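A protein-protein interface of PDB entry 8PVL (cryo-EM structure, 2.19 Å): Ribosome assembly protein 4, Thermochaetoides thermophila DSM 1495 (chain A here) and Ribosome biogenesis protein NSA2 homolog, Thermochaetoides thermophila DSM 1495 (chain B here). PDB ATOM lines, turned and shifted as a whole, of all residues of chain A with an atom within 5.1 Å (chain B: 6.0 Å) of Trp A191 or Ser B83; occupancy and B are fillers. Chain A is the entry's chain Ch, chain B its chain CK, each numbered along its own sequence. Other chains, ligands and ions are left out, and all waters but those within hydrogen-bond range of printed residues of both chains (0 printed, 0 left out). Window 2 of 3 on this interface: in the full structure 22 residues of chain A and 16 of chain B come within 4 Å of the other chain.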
ATOM      1  N   LEU A 150      16.689   8.052 -12.314  1.00  0.00           N
ATOM      2  CA  LEU A 150      16.355   7.890 -10.908  1.00  0.00           C
ATOM      3  C   LEU A 150      17.454   7.242 -10.085  1.00  0.00           C
ATOM      4  O   LEU A 150      17.538   7.506  -8.885  1.00  0.00           O
ATOM      5  CB  LEU A 150      15.065   7.073 -10.762  1.00  0.00           C
ATOM      6  CG  LEU A 150      13.939   7.499 -11.709  1.00  0.00           C
ATOM      7  CD1 LEU A 150      12.735   6.591 -11.565  1.00  0.00           C
ATOM      8  CD2 LEU A 150      13.549   8.949 -11.469  1.00  0.00           C
ATOM      9  N   SER A 166      16.077   4.440 -15.004  1.00  0.00           N
ATOM     10  CA  SER A 166      15.255   5.610 -15.274  1.00  0.00           C
ATOM     11  C   SER A 166      13.773   5.272 -15.199  1.00  0.00           C
ATOM     12  O   SER A 166      13.375   4.118 -15.026  1.00  0.00           O
ATOM     13  CB  SER A 166      15.583   6.206 -16.647  1.00  0.00           C
ATOM     14  OG  SER A 166      14.730   7.291 -16.956  1.00  0.00           O
ATOM     15  N   GLY A 167      12.960   6.316 -15.342  1.00  0.00           N
ATOM     16  CA  GLY A 167      11.519   6.225 -15.367  1.00  0.00           C
ATOM     17  C   GLY A 167      10.919   5.785 -16.679  1.00  0.00           C
ATOM     18  O   GLY A 167       9.694   5.666 -16.777  1.00  0.00           O
ATOM     19  N   ASN A 169      11.253   2.854 -17.731  1.00  0.00           N
ATOM     20  CA  ASN A 169      11.201   1.418 -17.478  1.00  0.00           C
ATOM     21  C   ASN A 169      12.441   0.680 -17.961  1.00  0.00           C
ATOM     22  O   ASN A 169      12.392  -0.533 -18.178  1.00  0.00           O
ATOM     23  CB  ASN A 169       9.941   0.784 -18.085  1.00  0.00           C
ATOM     24  CG  ASN A 169       8.681   1.538 -17.724  1.00  0.00           C
ATOM     25  OD1 ASN A 169       8.730   2.557 -17.038  1.00  0.00           O
ATOM     26  ND2 ASN A 169       7.542   1.044 -18.187  1.00  0.00           N
ATOM     27  N   THR A 189       8.071  -3.007 -16.377  1.00  0.00           N
ATOM     28  CA  THR A 189       6.908  -2.241 -16.808  1.00  0.00           C
ATOM     29  C   THR A 189       6.619  -1.068 -15.877  1.00  0.00           C
ATOM     30  O   THR A 189       5.541  -0.471 -15.949  1.00  0.00           O
ATOM     31  CB  THR A 189       5.682  -3.147 -16.931  1.00  0.00           C
ATOM     32  OG1 THR A 189       5.368  -3.717 -15.656  1.00  0.00           O
ATOM     33  CG2 THR A 189       5.949  -4.266 -17.927  1.00  0.00           C
ATOM     34  N   GLY A 190       7.564  -0.733 -14.998  1.00  0.00           N
ATOM     35  CA  GLY A 190       7.478   0.450 -14.166  1.00  0.00           C
ATOM     36  C   GLY A 190       8.836   1.119 -14.097  1.00  0.00           C
ATOM     37  O   GLY A 190       9.810   0.623 -14.663  1.00  0.00           O
ATOM     38  N   TRP A 191       8.884   2.255 -13.397  1.00  0.00           N
ATOM     39  CA  TRP A 191      10.127   3.010 -13.277  1.00  0.00           C
ATOM     40  C   TRP A 191      11.179   2.193 -12.543  1.00  0.00           C
ATOM     41  O   TRP A 191      10.911   1.639 -11.475  1.00  0.00           O
ATOM     42  CB  TRP A 191       9.911   4.320 -12.519  1.00  0.00           C
ATOM     43  CG  TRP A 191       8.717   5.132 -12.889  1.00  0.00           C
ATOM     44  CD1 TRP A 191       8.088   5.187 -14.095  1.00  0.00           C
ATOM     45  CD2 TRP A 191       8.020   6.040 -12.032  1.00  0.00           C
ATOM     46  NE1 TRP A 191       7.032   6.060 -14.038  1.00  0.00           N
ATOM     47  CE2 TRP A 191       6.970   6.599 -12.781  1.00  0.00           C
ATOM     48  CE3 TRP A 191       8.179   6.428 -10.698  1.00  0.00           C
ATOM     49  CZ2 TRP A 191       6.084   7.526 -12.242  1.00  0.00           C
ATOM     50  CZ3 TRP A 191       7.298   7.346 -10.166  1.00  0.00           C
ATOM     51  CH2 TRP A 191       6.263   7.885 -10.936  1.00  0.00           C
ATOM     52  N   VAL A 192      12.387   2.143 -13.099  1.00  0.00           N
ATOM     53  CA  VAL A 192      13.487   1.421 -12.467  1.00  0.00           C
ATOM     54  C   VAL A 192      14.004   2.306 -11.337  1.00  0.00           C
ATOM     55  O   VAL A 192      14.808   3.213 -11.557  1.00  0.00           O
ATOM     56  CB  VAL A 192      14.590   1.063 -13.466  1.00  0.00           C
ATOM     57  CG1 VAL A 192      15.720   0.320 -12.771  1.00  0.00           C
ATOM     58  CG2 VAL A 192      14.024   0.228 -14.600  1.00  0.00           C
ATOM     59  N   LEU A 193      13.523   2.053 -10.119  1.00  0.00           N
ATOM     60  CA  LEU A 193      13.893   2.875  -8.976  1.00  0.00           C
ATOM     61  C   LEU A 193      15.306   2.611  -8.487  1.00  0.00           C
ATOM     62  O   LEU A 193      15.913   3.505  -7.890  1.00  0.00           O
ATOM     63  CB  LEU A 193      12.920   2.655  -7.817  1.00  0.00           C
ATOM     64  CG  LEU A 193      11.455   3.012  -8.042  1.00  0.00           C
ATOM     65  CD1 LEU A 193      10.616   2.435  -6.923  1.00  0.00           C
ATOM     66  CD2 LEU A 193      11.284   4.518  -8.126  1.00  0.00           C
ATOM     67  N   CYS A 207      15.584  -2.864  -9.372  1.00  0.00           N
ATOM     68  CA  CYS A 207      14.301  -2.943  -8.688  1.00  0.00           C
ATOM     69  C   CYS A 207      13.398  -1.845  -9.223  1.00  0.00           C
ATOM     70  O   CYS A 207      13.842  -0.704  -9.418  1.00  0.00           O
ATOM     71  CB  CYS A 207      14.453  -2.819  -7.168  1.00  0.00           C
ATOM     72  SG  CYS A 207      15.014  -1.220  -6.539  1.00  0.00           S
ATOM     73  N   SER A 208      12.136  -2.192  -9.472  1.00  0.00           N
ATOM     74  CA  SER A 208      11.264  -1.268 -10.180  1.00  0.00           C
ATOM     75  C   SER A 208       9.917  -1.111  -9.486  1.00  0.00           C
ATOM     76  O   SER A 208       9.579  -1.830  -8.543  1.00  0.00           O
ATOM     77  CB  SER A 208      11.054  -1.712 -11.630  1.00  0.00           C
ATOM     78  OG  SER A 208       9.911  -1.093 -12.186  1.00  0.00           O
ATOM     79  N   MET A 209       9.148  -0.138  -9.986  1.00  0.00           N
ATOM     80  CA  MET A 209       7.795   0.147  -9.522  1.00  0.00           C
ATOM     81  C   MET A 209       6.795  -0.939  -9.885  1.00  0.00           C
ATOM     82  O   MET A 209       5.687  -0.936  -9.341  1.00  0.00           O
ATOM     83  CB  MET A 209       7.306   1.477 -10.103  1.00  0.00           C
ATOM     84  CG  MET A 209       8.005   2.709  -9.572  1.00  0.00           C
ATOM     85  SD  MET A 209       7.257   3.336  -8.059  1.00  0.00           S
ATOM     86  CE  MET A 209       5.866   4.244  -8.723  1.00  0.00           C
ATOM     87  N   PRO B  82       2.244   7.805  -9.075  1.00  0.00           N
ATOM     88  CA  PRO B  82       2.459   9.203  -9.454  1.00  0.00           C
ATOM     89  C   PRO B  82       2.517   9.386 -10.967  1.00  0.00           C
ATOM     90  O   PRO B  82       2.457   8.403 -11.704  1.00  0.00           O
ATOM     91  CB  PRO B  82       3.811   9.541  -8.810  1.00  0.00           C
ATOM     92  CG  PRO B  82       4.105   8.418  -7.830  1.00  0.00           C
ATOM     93  CD  PRO B  82       2.951   7.463  -7.832  1.00  0.00           C
ATOM     94  N   SER B  83       2.629  10.634 -11.421  1.00  0.00           N
ATOM     95  CA  SER B  83       2.669  10.941 -12.846  1.00  0.00           C
ATOM     96  C   SER B  83       4.095  11.141 -13.344  1.00  0.00           C
ATOM     97  O   SER B  83       4.548  10.431 -14.246  1.00  0.00           O
ATOM     98  CB  SER B  83       1.819  12.185 -13.140  1.00  0.00           C
ATOM     99  OG  SER B  83       0.473  11.991 -12.744  1.00  0.00           O
ATOM    100  N   ASP B  84       4.814  12.098 -12.768  1.00  0.00           N
ATOM    101  CA  ASP B  84       6.206  12.305 -13.143  1.00  0.00           C
ATOM    102  C   ASP B  84       7.096  11.293 -12.426  1.00  0.00           C
ATOM    103  O   ASP B  84       6.900  11.031 -11.236  1.00  0.00           O
ATOM    104  CB  ASP B  84       6.653  13.721 -12.797  1.00  0.00           C
ATOM    105  CG  ASP B  84       6.207  14.740 -13.824  1.00  0.00           C
ATOM    106  OD1 ASP B  84       6.238  15.948 -13.515  1.00  0.00           O
ATOM    107  OD2 ASP B  84       5.824  14.331 -14.941  1.00  0.00           O
ATOM    108  N   PRO B  85       8.065  10.700 -13.126  1.00  0.00           N
ATOM    109  CA  PRO B  85       8.997   9.778 -12.462  1.00  0.00           C
ATOM    110  C   PRO B  85       9.879  10.515 -11.464  1.00  0.00           C
ATOM    111  O   PRO B  85      10.446  11.565 -11.768  1.00  0.00           O
ATOM    112  CB  PRO B  85       9.815   9.198 -13.623  1.00  0.00           C
ATOM    113  CG  PRO B  85       8.987   9.455 -14.845  1.00  0.00           C
ATOM    114  CD  PRO B  85       8.275  10.741 -14.582  1.00  0.00           C
ATOM    115  N   ILE B  86       9.983   9.950 -10.266  1.00  0.00           N
ATOM    116  CA  ILE B  86      10.733  10.546  -9.162  1.00  0.00           C
ATOM    117  C   ILE B  86      11.538   9.438  -8.496  1.00  0.00           C
ATOM    118  O   ILE B  86      11.212   8.250  -8.645  1.00  0.00           O
ATOM    119  CB  ILE B  86       9.793  11.250  -8.152  1.00  0.00           C
ATOM    120  CG1 ILE B  86       8.550  10.402  -7.883  1.00  0.00           C
ATOM    121  CG2 ILE B  86       9.421  12.637  -8.647  1.00  0.00           C
ATOM    122  CD1 ILE B  86       7.731  10.885  -6.711  1.00  0.00           C
ATOM    123  N   LEU B  91       9.206   9.476  -3.140  1.00  0.00           N
ATOM    124  CA  LEU B  91       7.909   8.820  -3.193  1.00  0.00           C
ATOM    125  C   LEU B  91       7.109   9.114  -1.929  1.00  0.00           C
ATOM    126  O   LEU B  91       7.669   9.372  -0.859  1.00  0.00           O
ATOM    127  CB  LEU B  91       8.079   7.311  -3.364  1.00  0.00           C
ATOM    128  CG  LEU B  91       8.445   6.809  -4.762  1.00  0.00           C
ATOM    129  CD1 LEU B  91       8.751   5.325  -4.731  1.00  0.00           C
ATOM    130  CD2 LEU B  91       7.325   7.102  -5.738  1.00  0.00           C
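Printed residues of chain A that touch a printed residue of chain B: Leu A150, Gly A167, Trp A191 and Leu A193.
Hydrophobic or aromatic side chains of chain A that line the printed part of chain B: Leu A150, Trp A191 and Leu A193.
Printed residues of chain B that touch a printed residue of chain A: Pro B82, Ser B83, Asp B84, Pro B85 and Ile B86.
Hydrophobic or aromatic side chains of chain B within 4 Å of the printed part of chain A: Pro B82 and Pro B85.
Among the printed residues, no Asp or Glu carboxylate lies within 4 Å of a Lys or Arg side-chain nitrogen of the other chain.
Trp A191 touches just these residues of chain B: Pro B82, Ser B83, Asp B84, Pro B85 and Ile B86.
Ser B83 touches just one residue of chain A: Trp A191 (3.8 Å).
Printed residues of chain B within 4 Å of Leu A193: Ile B86 (3.8 Å).
Printed residues of chain A within 4 Å of Asp B84: Trp A191 (3.2 Å).
Of the printed residues of chain A, Ile B86 touches Leu A150 (3.6 Å), Trp A191 (3.7 Å) and Leu A193 (3.8 Å).
Of the printed residues of chain A, Pro B85 touches Leu A150, Gly A167 and Trp A191.
Gly A190 touches none of the printed residues of chain B.
The nearest residue of chain B that does not touch Trp A191 is Leu B91 (4.4 Å).
O of Trp A191 is in hydrogen-bond range of OG of Ser A208 (3.0 Å).
The backbone NH (N) of Met A209 sits at hydrogen-bond distance from the backbone carbonyl oxygen (O) of Trp A191, at 2.9 Å.
The backbone NH (N) of Leu A193 lies within hydrogen-bond range of the backbone carbonyl oxygen (O) of Cys A207 (2.9 Å).
OD1 of Asn A169 sits close to O of Gly A167 (3.3 Å).
C of Pro B85 touches CD2 of Leu A150, 3.99 Å away.
Ile B86 touches Leu A150.
CA of Gly A167 touches CB of Pro B85, 3.8 Å away.
Trp A191 touches Pro B82 (CH2 to CB, 3.6 Å).
Trp A191 touches Ser B83 (CZ2 to O, 3.8 Å).
Asp B84 touches Trp A191 (O to CH2, 3.2 Å).
Pro B85 touches Trp A191 (CA to CH2, 3.7 Å).
Trp A191 touches Ile B86 (CZ3 to N, 3.7 Å).
O of Ile B86 touches CD2 of Leu A193 (3.8 Å).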
